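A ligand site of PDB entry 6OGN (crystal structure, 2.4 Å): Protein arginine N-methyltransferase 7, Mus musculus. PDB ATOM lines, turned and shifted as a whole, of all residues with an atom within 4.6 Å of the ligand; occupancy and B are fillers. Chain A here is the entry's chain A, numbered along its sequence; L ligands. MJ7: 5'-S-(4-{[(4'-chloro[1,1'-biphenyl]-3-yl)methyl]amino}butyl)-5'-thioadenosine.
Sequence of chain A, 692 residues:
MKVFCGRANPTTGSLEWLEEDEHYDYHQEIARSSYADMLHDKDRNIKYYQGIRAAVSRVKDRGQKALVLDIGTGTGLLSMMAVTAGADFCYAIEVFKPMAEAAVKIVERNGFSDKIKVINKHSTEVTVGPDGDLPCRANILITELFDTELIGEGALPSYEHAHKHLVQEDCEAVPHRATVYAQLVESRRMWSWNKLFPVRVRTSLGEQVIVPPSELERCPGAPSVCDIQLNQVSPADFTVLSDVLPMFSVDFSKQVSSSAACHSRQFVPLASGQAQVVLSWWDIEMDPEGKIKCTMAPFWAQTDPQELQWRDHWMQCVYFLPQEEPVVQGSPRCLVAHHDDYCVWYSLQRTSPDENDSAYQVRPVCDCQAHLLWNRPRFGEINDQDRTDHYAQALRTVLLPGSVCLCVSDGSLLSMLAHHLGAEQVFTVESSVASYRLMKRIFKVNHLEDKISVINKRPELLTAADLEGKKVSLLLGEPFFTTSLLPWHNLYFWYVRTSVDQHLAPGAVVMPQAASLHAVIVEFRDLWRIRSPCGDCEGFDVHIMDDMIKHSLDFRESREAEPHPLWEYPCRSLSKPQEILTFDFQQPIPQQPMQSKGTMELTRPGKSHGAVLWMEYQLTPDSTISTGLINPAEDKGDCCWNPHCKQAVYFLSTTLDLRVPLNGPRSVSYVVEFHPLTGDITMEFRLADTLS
The backbone carbonyl oxygen (O) of Phe 146 sits close to a nitrogen (N5) of the ligand.
The backbone NH (N) of Ser 123 sits at hydrogen-bond distance from a nitrogen (N1) of the ligand (2.9 Å).
N of the ligand lies within hydrogen-bond range of OG of Ser 123, 2.9 Å away.
The backbone NH (N) of Val 95 sits at hydrogen-bond distance from a nitrogen (N2) of the ligand (3.3 Å).
A ring nitrogen (NE2) of His 122 lies close to a nitrogen (N) of the ligand (3.4 Å).
The side-chain hydroxyl (OG) of Ser 158 is in hydrogen-bond range of a nitrogen (N) of the ligand, 3.0 Å away.
An oxygen (O1) of the ligand sits at hydrogen-bond distance from the side-chain carboxylate (OE1) of Glu 94, at 2.6 Å.
The backbone NH (N) of Ile 284 lies within hydrogen-bond range of the backbone carbonyl oxygen (O) of Cys 294, at 2.8 Å.
O of Lys 121 sits at hydrogen-bond distance from N of Val 95 (3.4 Å).
The backbone carbonyl oxygen of Glu 94 lies within hydrogen-bond range of the backbone NH of Lys 121, 3.3 Å away.
NE1 of Trp 282 is in hydrogen-bond range of O of Thr 148.
The backbone carbonyl oxygen of Trp 282 lies within hydrogen-bond range of the backbone NH of Met 296 (3.0 Å).
NE1 of Trp 282 is in hydrogen-bond range of O of Asp 147.
The side-chain carboxylate of Glu 94 is in hydrogen-bond range of the backbone NH of Gly 74, at 3.1 Å.
The backbone NH (N) of Phe 96 sits at hydrogen-bond distance from the side-chain carboxylate (OE2) of Glu 94 (3.2 Å).
CE1 of Tyr 35 touches O1 of the ligand, 3.3 Å away.
CG of Arg 44 touches C23 of the ligand, 3.8 Å away.
CE2 of Tyr 48 touches CL of the ligand, 3.7 Å away.
Ile 71 touches the ligand.
CA of Gly 72 touches O2 of the ligand (3.0 Å).
Ile 93 touches the ligand (CG2 to C1, 3.9 Å).
Lys 121 touches the ligand.
Leu 145 touches the ligand.
CG of Glu 153 touches C10 of the ligand (3.997 Å).
CH2 of Trp 282 touches C20 of the ligand, 3.7 Å away.
Ile 284 touches the ligand (CG1 to CL, 3.5 Å).
Met 286 touches the ligand (CE to CL, 3.2 Å).
Cys 294 touches the ligand (SG to CL, 3.6 Å).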
ATOM      1  N   TYR A  35       5.174 -21.686 -32.922  1.00  0.00           N
ATOM      2  CA  TYR A  35       4.865 -20.339 -32.342  1.00  0.00           C
ATOM      3  C   TYR A  35       3.976 -19.537 -33.302  1.00  0.00           C
ATOM      4  O   TYR A  35       3.675 -18.374 -32.999  1.00  0.00           O
ATOM      5  CB  TYR A  35       6.157 -19.568 -32.028  1.00  0.00           C
ATOM      6  CG  TYR A  35       7.338 -20.425 -31.633  1.00  0.00           C
ATOM      7  CD1 TYR A  35       7.616 -20.690 -30.304  1.00  0.00           C
ATOM      8  CD2 TYR A  35       8.189 -20.945 -32.592  1.00  0.00           C
ATOM      9  CE1 TYR A  35       8.712 -21.468 -29.941  1.00  0.00           C
ATOM     10  CE2 TYR A  35       9.280 -21.724 -32.251  1.00  0.00           C
ATOM     11  CZ  TYR A  35       9.544 -21.985 -30.914  1.00  0.00           C
ATOM     12  OH  TYR A  35      10.621 -22.746 -30.571  1.00  0.00           O
ATOM     13  N   ASP A  41      -4.426 -17.633 -31.695  1.00  0.00           N
ATOM     14  CA  ASP A  41      -5.324 -17.964 -30.559  1.00  0.00           C
ATOM     15  C   ASP A  41      -5.732 -16.667 -29.846  1.00  0.00           C
ATOM     16  O   ASP A  41      -5.139 -16.335 -28.782  1.00  0.00           O
ATOM     17  CB  ASP A  41      -4.676 -18.985 -29.611  1.00  0.00           C
ATOM     18  CG  ASP A  41      -5.682 -19.763 -28.760  1.00  0.00           C
ATOM     19  OD1 ASP A  41      -6.893 -19.436 -28.825  1.00  0.00           O
ATOM     20  OD2 ASP A  41      -5.241 -20.697 -28.031  1.00  0.00           O
ATOM     21  N   ARG A  44      -6.857 -17.088 -26.103  1.00  0.00           N
ATOM     22  CA  ARG A  44      -5.630 -17.166 -25.245  1.00  0.00           C
ATOM     23  C   ARG A  44      -5.091 -15.729 -25.034  1.00  0.00           C
ATOM     24  O   ARG A  44      -4.976 -15.306 -23.866  1.00  0.00           O
ATOM     25  CB  ARG A  44      -4.620 -18.103 -25.912  1.00  0.00           C
ATOM     26  CG  ARG A  44      -3.343 -18.370 -25.136  1.00  0.00           C
ATOM     27  CD  ARG A  44      -2.394 -19.167 -26.010  1.00  0.00           C
ATOM     28  NE  ARG A  44      -0.975 -18.988 -25.731  1.00  0.00           N
ATOM     29  CZ  ARG A  44      -0.299 -17.854 -25.912  1.00  0.00           C
ATOM     30  NH1 ARG A  44       0.998 -17.809 -25.638  1.00  0.00           N
ATOM     31  NH2 ARG A  44      -0.908 -16.758 -26.348  1.00  0.00           N
ATOM     32  N   TYR A  48      -4.915 -13.650 -21.435  1.00  0.00           N
ATOM     33  CA  TYR A  48      -3.572 -13.204 -20.934  1.00  0.00           C
ATOM     34  C   TYR A  48      -3.621 -11.678 -20.758  1.00  0.00           C
ATOM     35  O   TYR A  48      -3.335 -11.200 -19.654  1.00  0.00           O
ATOM     36  CB  TYR A  48      -2.448 -13.651 -21.852  1.00  0.00           C
ATOM     37  CG  TYR A  48      -1.830 -14.969 -21.462  1.00  0.00           C
ATOM     38  CD1 TYR A  48      -0.997 -15.058 -20.368  1.00  0.00           C
ATOM     39  CD2 TYR A  48      -2.081 -16.120 -22.173  1.00  0.00           C
ATOM     40  CE1 TYR A  48      -0.434 -16.255 -19.984  1.00  0.00           C
ATOM     41  CE2 TYR A  48      -1.523 -17.323 -21.819  1.00  0.00           C
ATOM     42  CZ  TYR A  48      -0.682 -17.389 -20.725  1.00  0.00           C
ATOM     43  OH  TYR A  48      -0.101 -18.570 -20.371  1.00  0.00           O
ATOM     44  N   ILE A  71       8.690 -15.802 -18.410  1.00  0.00           N
ATOM     45  CA  ILE A  71       9.441 -17.027 -18.799  1.00  0.00           C
ATOM     46  C   ILE A  71       8.780 -17.643 -20.049  1.00  0.00           C
ATOM     47  O   ILE A  71       7.626 -18.140 -19.958  1.00  0.00           O
ATOM     48  CB  ILE A  71       9.520 -18.029 -17.637  1.00  0.00           C
ATOM     49  CG1 ILE A  71      10.054 -17.391 -16.368  1.00  0.00           C
ATOM     50  CG2 ILE A  71      10.338 -19.227 -18.036  1.00  0.00           C
ATOM     51  CD1 ILE A  71       9.807 -18.205 -15.134  1.00  0.00           C
ATOM     52  N   GLY A  72       9.528 -17.636 -21.164  1.00  0.00           N
ATOM     53  CA  GLY A  72       9.146 -18.239 -22.444  1.00  0.00           C
ATOM     54  C   GLY A  72       8.494 -17.220 -23.335  1.00  0.00           C
ATOM     55  O   GLY A  72       7.437 -17.507 -23.904  1.00  0.00           O
ATOM     56  N   GLY A  74       8.778 -15.952 -26.158  1.00  0.00           N
ATOM     57  CA  GLY A  74       8.612 -16.068 -27.628  1.00  0.00           C
ATOM     58  C   GLY A  74       8.868 -14.732 -28.317  1.00  0.00           C
ATOM     59  O   GLY A  74      10.045 -14.304 -28.384  1.00  0.00           O
ATOM     60  N   ILE A  93      12.437 -13.879 -20.699  1.00  0.00           N
ATOM     61  CA  ILE A  93      13.379 -15.024 -20.806  1.00  0.00           C
ATOM     62  C   ILE A  93      12.976 -15.889 -22.012  1.00  0.00           C
ATOM     63  O   ILE A  93      11.801 -16.256 -22.110  1.00  0.00           O
ATOM     64  CB  ILE A  93      13.419 -15.824 -19.501  1.00  0.00           C
ATOM     65  CG1 ILE A  93      13.350 -14.948 -18.240  1.00  0.00           C
ATOM     66  CG2 ILE A  93      14.630 -16.734 -19.480  1.00  0.00           C
ATOM     67  CD1 ILE A  93      14.433 -13.889 -18.122  1.00  0.00           C
ATOM     68  N   GLU A  94      13.939 -16.220 -22.871  1.00  0.00           N
ATOM     69  CA  GLU A  94      13.748 -17.082 -24.059  1.00  0.00           C
ATOM     70  C   GLU A  94      15.048 -17.833 -24.339  1.00  0.00           C
ATOM     71  O   GLU A  94      16.046 -17.159 -24.680  1.00  0.00           O
ATOM     72  CB  GLU A  94      13.319 -16.263 -25.278  1.00  0.00           C
ATOM     73  CG  GLU A  94      13.077 -17.101 -26.524  1.00  0.00           C
ATOM     74  CD  GLU A  94      12.151 -18.294 -26.369  1.00  0.00           C
ATOM     75  OE1 GLU A  94      10.975 -18.100 -25.941  1.00  0.00           O
ATOM     76  OE2 GLU A  94      12.589 -19.424 -26.660  1.00  0.00           O
ATOM     77  N   VAL A  95      15.031 -19.152 -24.207  1.00  0.00           N
ATOM     78  CA  VAL A  95      16.238 -20.017 -24.287  1.00  0.00           C
ATOM     79  C   VAL A  95      16.665 -20.206 -25.753  1.00  0.00           C
ATOM     80  O   VAL A  95      17.825 -20.509 -25.970  1.00  0.00           O
ATOM     81  CB  VAL A  95      15.996 -21.376 -23.608  1.00  0.00           C
ATOM     82  CG1 VAL A  95      14.926 -22.198 -24.302  1.00  0.00           C
ATOM     83  CG2 VAL A  95      17.285 -22.177 -23.494  1.00  0.00           C
ATOM     84  N   PHE A  96      15.745 -20.095 -26.705  1.00  0.00           N
ATOM     85  CA  PHE A  96      15.964 -20.394 -28.147  1.00  0.00           C
ATOM     86  C   PHE A  96      16.465 -19.127 -28.848  1.00  0.00           C
ATOM     87  O   PHE A  96      15.640 -18.212 -29.102  1.00  0.00           O
ATOM     88  CB  PHE A  96      14.673 -20.925 -28.760  1.00  0.00           C
ATOM     89  CG  PHE A  96      14.811 -21.516 -30.137  1.00  0.00           C
ATOM     90  CD1 PHE A  96      15.745 -22.514 -30.396  1.00  0.00           C
ATOM     91  CD2 PHE A  96      14.011 -21.091 -31.185  1.00  0.00           C
ATOM     92  CE1 PHE A  96      15.886 -23.059 -31.662  1.00  0.00           C
ATOM     93  CE2 PHE A  96      14.160 -21.618 -32.459  1.00  0.00           C
ATOM     94  CZ  PHE A  96      15.094 -22.603 -32.692  1.00  0.00           C
ATOM     95  N   LYS A 121      18.401 -17.198 -22.377  1.00  0.00           N
ATOM     96  CA  LYS A 121      18.827 -18.288 -21.470  1.00  0.00           C
ATOM     97  C   LYS A 121      17.616 -19.127 -21.088  1.00  0.00           C
ATOM     98  O   LYS A 121      16.488 -18.639 -21.163  1.00  0.00           O
ATOM     99  CB  LYS A 121      19.453 -17.751 -20.193  1.00  0.00           C
ATOM    100  CG  LYS A 121      20.808 -17.067 -20.347  1.00  0.00           C
ATOM    101  CD  LYS A 121      21.324 -16.611 -19.000  1.00  0.00           C
ATOM    102  CE  LYS A 121      22.506 -15.671 -19.087  1.00  0.00           C
ATOM    103  NZ  LYS A 121      23.052 -15.405 -17.734  1.00  0.00           N
ATOM    104  N   HIS A 122      17.853 -20.342 -20.630  1.00  0.00           N
ATOM    105  CA  HIS A 122      16.874 -21.090 -19.826  1.00  0.00           C
ATOM    106  C   HIS A 122      16.660 -20.330 -18.525  1.00  0.00           C
ATOM    107  O   HIS A 122      17.665 -19.779 -17.977  1.00  0.00           O
ATOM    108  CB  HIS A 122      17.335 -22.531 -19.637  1.00  0.00           C
ATOM    109  CG  HIS A 122      16.207 -23.440 -19.284  1.00  0.00           C
ATOM    110  ND1 HIS A 122      15.785 -23.609 -17.998  1.00  0.00           N
ATOM    111  CD2 HIS A 122      15.410 -24.207 -20.051  1.00  0.00           C
ATOM    112  CE1 HIS A 122      14.776 -24.461 -17.970  1.00  0.00           C
ATOM    113  NE2 HIS A 122      14.521 -24.836 -19.213  1.00  0.00           N
ATOM    114  N   SER A 123      15.415 -20.263 -18.048  1.00  0.00           N
ATOM    115  CA  SER A 123      15.042 -19.517 -16.824  1.00  0.00           C
ATOM    116  C   SER A 123      15.847 -20.040 -15.638  1.00  0.00           C
ATOM    117  O   SER A 123      16.157 -19.235 -14.764  1.00  0.00           O
ATOM    118  CB  SER A 123      13.558 -19.560 -16.570  1.00  0.00           C
ATOM    119  OG  SER A 123      13.107 -20.865 -16.306  1.00  0.00           O
ATOM    120  N   GLU A 144       3.872 -18.992 -20.485  1.00  0.00           N
ATOM    121  CA  GLU A 144       3.022 -19.814 -21.373  1.00  0.00           C
ATOM    122  C   GLU A 144       3.682 -21.193 -21.610  1.00  0.00           C
ATOM    123  O   GLU A 144       3.630 -21.688 -22.718  1.00  0.00           O
ATOM    124  CB  GLU A 144       2.760 -19.044 -22.672  1.00  0.00           C
ATOM    125  CG  GLU A 144       1.317 -19.165 -23.160  1.00  0.00           C
ATOM    126  N   LEU A 145       4.200 -21.817 -20.574  1.00  0.00           N
ATOM    127  CA  LEU A 145       4.980 -23.080 -20.696  1.00  0.00           C
ATOM    128  C   LEU A 145       4.060 -24.310 -20.566  1.00  0.00           C
ATOM    129  O   LEU A 145       4.381 -25.239 -19.834  1.00  0.00           O
ATOM    130  CB  LEU A 145       6.032 -23.064 -19.601  1.00  0.00           C
ATOM    131  CG  LEU A 145       6.945 -21.858 -19.653  1.00  0.00           C
ATOM    132  CD1 LEU A 145       7.657 -21.688 -18.334  1.00  0.00           C
ATOM    133  CD2 LEU A 145       7.928 -21.986 -20.802  1.00  0.00           C
ATOM    134  N   PHE A 146       2.967 -24.335 -21.301  1.00  0.00           N
ATOM    135  CA  PHE A 146       1.938 -25.389 -21.174  1.00  0.00           C
ATOM    136  C   PHE A 146       1.768 -26.092 -22.518  1.00  0.00           C
ATOM    137  O   PHE A 146       1.792 -25.422 -23.544  1.00  0.00           O
ATOM    138  CB  PHE A 146       0.647 -24.781 -20.655  1.00  0.00           C
ATOM    139  CG  PHE A 146       0.875 -23.964 -19.421  1.00  0.00           C
ATOM    140  CD1 PHE A 146       1.307 -24.574 -18.262  1.00  0.00           C
ATOM    141  CD2 PHE A 146       0.701 -22.596 -19.428  1.00  0.00           C
ATOM    142  CE1 PHE A 146       1.530 -23.829 -17.126  1.00  0.00           C
ATOM    143  CE2 PHE A 146       0.930 -21.857 -18.289  1.00  0.00           C
ATOM    144  CZ  PHE A 146       1.356 -22.465 -17.142  1.00  0.00           C
ATOM    145  N   ASP A 147       1.644 -27.410 -22.470  1.00  0.00           N
ATOM    146  CA  ASP A 147       1.210 -28.247 -23.624  1.00  0.00           C
ATOM    147  C   ASP A 147      -0.131 -28.897 -23.240  1.00  0.00           C
ATOM    148  O   ASP A 147      -0.652 -28.588 -22.129  1.00  0.00           O
ATOM    149  CB  ASP A 147       2.301 -29.259 -23.993  1.00  0.00           C
ATOM    150  CG  ASP A 147       2.640 -30.275 -22.903  1.00  0.00           C
ATOM    151  OD1 ASP A 147       2.077 -30.159 -21.775  1.00  0.00           O
ATOM    152  OD2 ASP A 147       3.484 -31.160 -23.178  1.00  0.00           O
ATOM    153  N   THR A 148      -0.636 -29.768 -24.111  1.00  0.00           N
ATOM    154  CA  THR A 148      -1.855 -30.595 -23.915  1.00  0.00           C
ATOM    155  C   THR A 148      -1.834 -31.292 -22.549  1.00  0.00           C
ATOM    156  O   THR A 148      -2.845 -31.260 -21.889  1.00  0.00           O
ATOM    157  CB  THR A 148      -1.996 -31.554 -25.097  1.00  0.00           C
ATOM    158  OG1 THR A 148      -2.051 -30.723 -26.262  1.00  0.00           O
ATOM    159  CG2 THR A 148      -3.223 -32.416 -25.006  1.00  0.00           C
ATOM    160  N   GLU A 153       5.991 -29.429 -20.902  1.00  0.00           N
ATOM    161  CA  GLU A 153       7.032 -28.470 -21.395  1.00  0.00           C
ATOM    162  C   GLU A 153       7.821 -27.858 -20.238  1.00  0.00           C
ATOM    163  O   GLU A 153       8.549 -26.879 -20.497  1.00  0.00           O
ATOM    164  CB  GLU A 153       6.397 -27.376 -22.256  1.00  0.00           C
ATOM    165  CG  GLU A 153       5.735 -27.908 -23.515  1.00  0.00           C
ATOM    166  CD  GLU A 153       6.679 -28.445 -24.586  1.00  0.00           C
ATOM    167  OE1 GLU A 153       6.191 -28.904 -25.628  1.00  0.00           O
ATOM    168  OE2 GLU A 153       7.908 -28.417 -24.361  1.00  0.00           O
ATOM    169  N   SER A 158      10.434 -25.161 -14.001  1.00  0.00           N
ATOM    170  CA  SER A 158      10.591 -23.697 -14.277  1.00  0.00           C
ATOM    171  C   SER A 158       9.933 -22.867 -13.163  1.00  0.00           C
ATOM    172  O   SER A 158      10.610 -21.936 -12.650  1.00  0.00           O
ATOM    173  CB  SER A 158      10.077 -23.352 -15.621  1.00  0.00           C
ATOM    174  OG  SER A 158      10.830 -24.014 -16.614  1.00  0.00           O
ATOM    175  N   TRP A 282      -7.190 -29.675 -19.193  1.00  0.00           N
ATOM    176  CA  TRP A 282      -7.032 -28.727 -18.060  1.00  0.00           C
ATOM    177  C   TRP A 282      -7.773 -27.451 -18.368  1.00  0.00           C
ATOM    178  O   TRP A 282      -8.168 -27.268 -19.536  1.00  0.00           O
ATOM    179  CB  TRP A 282      -5.557 -28.443 -17.764  1.00  0.00           C
ATOM    180  CG  TRP A 282      -4.715 -28.191 -18.975  1.00  0.00           C
ATOM    181  CD1 TRP A 282      -4.123 -29.129 -19.759  1.00  0.00           C
ATOM    182  CD2 TRP A 282      -4.345 -26.928 -19.534  1.00  0.00           C
ATOM    183  NE1 TRP A 282      -3.459 -28.546 -20.784  1.00  0.00           N
ATOM    184  CE2 TRP A 282      -3.530 -27.194 -20.644  1.00  0.00           C
ATOM    185  CE3 TRP A 282      -4.596 -25.589 -19.183  1.00  0.00           C
ATOM    186  CZ2 TRP A 282      -2.983 -26.180 -21.430  1.00  0.00           C
ATOM    187  CZ3 TRP A 282      -4.043 -24.594 -19.959  1.00  0.00           C
ATOM    188  CH2 TRP A 282      -3.265 -24.886 -21.080  1.00  0.00           C
ATOM    189  N   ILE A 284      -7.276 -23.025 -17.134  1.00  0.00           N
ATOM    190  CA  ILE A 284      -6.411 -22.008 -16.489  1.00  0.00           C
ATOM    191  C   ILE A 284      -7.320 -20.898 -15.982  1.00  0.00           C
ATOM    192  O   ILE A 284      -8.227 -20.478 -16.741  1.00  0.00           O
ATOM    193  CB  ILE A 284      -5.372 -21.417 -17.470  1.00  0.00           C
ATOM    194  CG1 ILE A 284      -5.772 -21.632 -18.932  1.00  0.00           C
ATOM    195  CG2 ILE A 284      -3.963 -21.940 -17.187  1.00  0.00           C
ATOM    196  N   MET A 286      -6.701 -16.844 -14.915  1.00  0.00           N
ATOM    197  CA  MET A 286      -5.698 -15.780 -15.171  1.00  0.00           C
ATOM    198  C   MET A 286      -5.600 -14.810 -13.974  1.00  0.00           C
ATOM    199  O   MET A 286      -4.573 -14.065 -13.847  1.00  0.00           O
ATOM    200  CB  MET A 286      -6.092 -15.027 -16.434  1.00  0.00           C
ATOM    201  CG  MET A 286      -6.111 -15.905 -17.652  1.00  0.00           C
ATOM    202  SD  MET A 286      -4.447 -16.469 -18.089  1.00  0.00           S
ATOM    203  CE  MET A 286      -4.763 -17.187 -19.700  1.00  0.00           C
ATOM    204  N   CYS A 294      -9.679 -19.943 -19.491  1.00  0.00           N
ATOM    205  CA  CYS A 294      -9.698 -20.799 -20.697  1.00  0.00           C
ATOM    206  C   CYS A 294      -9.790 -22.244 -20.226  1.00  0.00           C
ATOM    207  O   CYS A 294      -9.152 -22.573 -19.210  1.00  0.00           O
ATOM    208  CB  CYS A 294      -8.436 -20.688 -21.564  1.00  0.00           C
ATOM    209  SG  CYS A 294      -7.752 -19.026 -21.684  1.00  0.00           S
ATOM    210  N   MET A 296      -9.682 -26.436 -21.956  1.00  0.00           N
ATOM    211  CA  MET A 296      -9.422 -27.327 -23.112  1.00  0.00           C
ATOM    212  C   MET A 296     -10.546 -28.389 -23.163  1.00  0.00           C
ATOM    213  O   MET A 296     -10.530 -29.237 -24.059  1.00  0.00           O
ATOM    214  CB  MET A 296      -8.048 -27.981 -22.955  1.00  0.00           C
ATOM    215  CG  MET A 296      -6.964 -27.494 -23.961  1.00  0.00           C
ATOM    216  SD  MET A 296      -6.654 -25.722 -24.016  1.00  0.00           S
ATOM    217  CE  MET A 296      -6.458 -25.370 -22.272  1.00  0.00           C
ATOM    218  N   ARG A 311      -8.400 -25.238 -30.676  1.00  0.00           N
ATOM    219  CA  ARG A 311      -7.019 -25.195 -30.084  1.00  0.00           C
ATOM    220  C   ARG A 311      -6.040 -26.099 -30.881  1.00  0.00           C
ATOM    221  O   ARG A 311      -6.457 -27.214 -31.315  1.00  0.00           O
ATOM    222  CB  ARG A 311      -7.091 -25.561 -28.597  1.00  0.00           C
ATOM    223  CG  ARG A 311      -6.197 -24.695 -27.708  1.00  0.00           C
ATOM    224  CD  ARG A 311      -6.732 -23.298 -27.408  1.00  0.00           C
ATOM    225  NE  ARG A 311      -7.870 -23.315 -26.504  1.00  0.00           N
ATOM    226  CZ  ARG A 311      -8.386 -22.257 -25.878  1.00  0.00           C
ATOM    227  NH1 ARG A 311      -7.843 -21.056 -26.031  1.00  0.00           N
ATOM    228  NH2 ARG A 311      -9.439 -22.406 -25.096  1.00  0.00           N
ATOM    229  N   ASP A 312      -4.794 -25.614 -31.074  1.00  0.00           N
ATOM    230  CA  ASP A 312      -3.653 -26.348 -31.704  1.00  0.00           C
ATOM    231  C   ASP A 312      -2.492 -26.419 -30.717  1.00  0.00           C
ATOM    232  O   ASP A 312      -2.093 -27.550 -30.361  1.00  0.00           O
ATOM    233  CB  ASP A 312      -3.218 -25.678 -33.016  1.00  0.00           C
ATOM    234  N   MET A 315      -5.163 -29.206 -27.364  1.00  0.00           N
ATOM    235  CA  MET A 315      -6.268 -30.196 -27.506  1.00  0.00           C
ATOM    236  C   MET A 315      -6.365 -31.044 -26.215  1.00  0.00           C
ATOM    237  O   MET A 315      -6.050 -30.482 -25.141  1.00  0.00           O
ATOM    238  CB  MET A 315      -6.059 -31.076 -28.747  1.00  0.00           C
ATOM    239  CG  MET A 315      -4.697 -31.755 -28.836  1.00  0.00           C
ATOM    240  SD  MET A 315      -4.343 -32.431 -30.532  1.00  0.00           S
ATOM    241  CE  MET A 315      -3.034 -31.319 -31.046  1.00  0.00           C
HETATM  242  C8  MJ7 L   1       8.400 -20.796 -25.156  1.00  0.00           C
HETATM  243  C13 MJ7 L   1       3.283 -24.702 -26.271  1.00  0.00           C
HETATM  244  C12 MJ7 L   1       4.471 -24.054 -26.995  1.00  0.00           C
HETATM  245  C11 MJ7 L   1       5.840 -24.476 -26.451  1.00  0.00           C
HETATM  246  C10 MJ7 L   1       6.001 -24.193 -24.965  1.00  0.00           C
HETATM  247  C9  MJ7 L   1       7.118 -21.599 -24.940  1.00  0.00           C
HETATM  248  C25 MJ7 L   1      -3.853 -22.646 -24.244  1.00  0.00           C
HETATM  249  C26 MJ7 L   1      -0.772 -23.889 -25.751  1.00  0.00           C
HETATM  250  C19 MJ7 L   1      -1.944 -24.076 -25.021  1.00  0.00           C
HETATM  251  C20 MJ7 L   1      -2.500 -22.978 -24.193  1.00  0.00           C
HETATM  252  C21 MJ7 L   1      -1.703 -22.285 -23.288  1.00  0.00           C
HETATM  253  C22 MJ7 L   1      -2.236 -21.339 -22.428  1.00  0.00           C
HETATM  254  C23 MJ7 L   1      -3.583 -21.044 -22.505  1.00  0.00           C
HETATM  255  C24 MJ7 L   1      -4.405 -21.684 -23.403  1.00  0.00           C
HETATM  256  C14 MJ7 L   1       1.063 -24.679 -27.297  1.00  0.00           C
HETATM  257  C15 MJ7 L   1      -0.275 -24.861 -26.622  1.00  0.00           C
HETATM  258  C16 MJ7 L   1      -1.014 -26.035 -26.792  1.00  0.00           C
HETATM  259  C17 MJ7 L   1      -2.179 -26.238 -26.077  1.00  0.00           C
HETATM  260  C18 MJ7 L   1      -2.629 -25.284 -25.184  1.00  0.00           C
HETATM  261  C2  MJ7 L   1      11.864 -21.370 -22.141  1.00  0.00           C
HETATM  262  C7  MJ7 L   1       9.305 -21.266 -26.306  1.00  0.00           C
HETATM  263  C6  MJ7 L   1      10.434 -22.013 -25.588  1.00  0.00           C
HETATM  264  C5  MJ7 L   1      10.526 -21.224 -24.278  1.00  0.00           C
HETATM  265  C4  MJ7 L   1      10.594 -23.099 -22.547  1.00  0.00           C
HETATM  266  C3  MJ7 L   1      11.753 -22.178 -21.027  1.00  0.00           C
HETATM  267 CL   MJ7 L   1      -4.260 -19.810 -21.458  1.00  0.00          CL
HETATM  268  N5  MJ7 L   1       2.038 -23.957 -26.457  1.00  0.00           N
HETATM  269  S   MJ7 L   1       7.532 -23.324 -24.533  1.00  0.00           S
HETATM  270  O1  MJ7 L   1       9.751 -20.140 -27.063  1.00  0.00           O
HETATM  271  O   MJ7 L   1      11.618 -21.917 -26.372  1.00  0.00           O
HETATM  272  O2  MJ7 L   1       9.210 -20.811 -23.965  1.00  0.00           O
HETATM  273  N4  MJ7 L   1      11.057 -21.937 -23.097  1.00  0.00           N
HETATM  274  N2  MJ7 L   1      12.611 -20.267 -22.259  1.00  0.00           N
HETATM  275  C1  MJ7 L   1      13.244 -19.989 -21.120  1.00  0.00           C
HETATM  276  N1  MJ7 L   1      13.197 -20.634 -19.951  1.00  0.00           N
HETATM  277  N3  MJ7 L   1      10.969 -23.287 -21.298  1.00  0.00           N
HETATM  278  C   MJ7 L   1      12.422 -21.743 -19.853  1.00  0.00           C
HETATM  279  N   MJ7 L   1      12.291 -22.326 -18.640  1.00  0.00           N
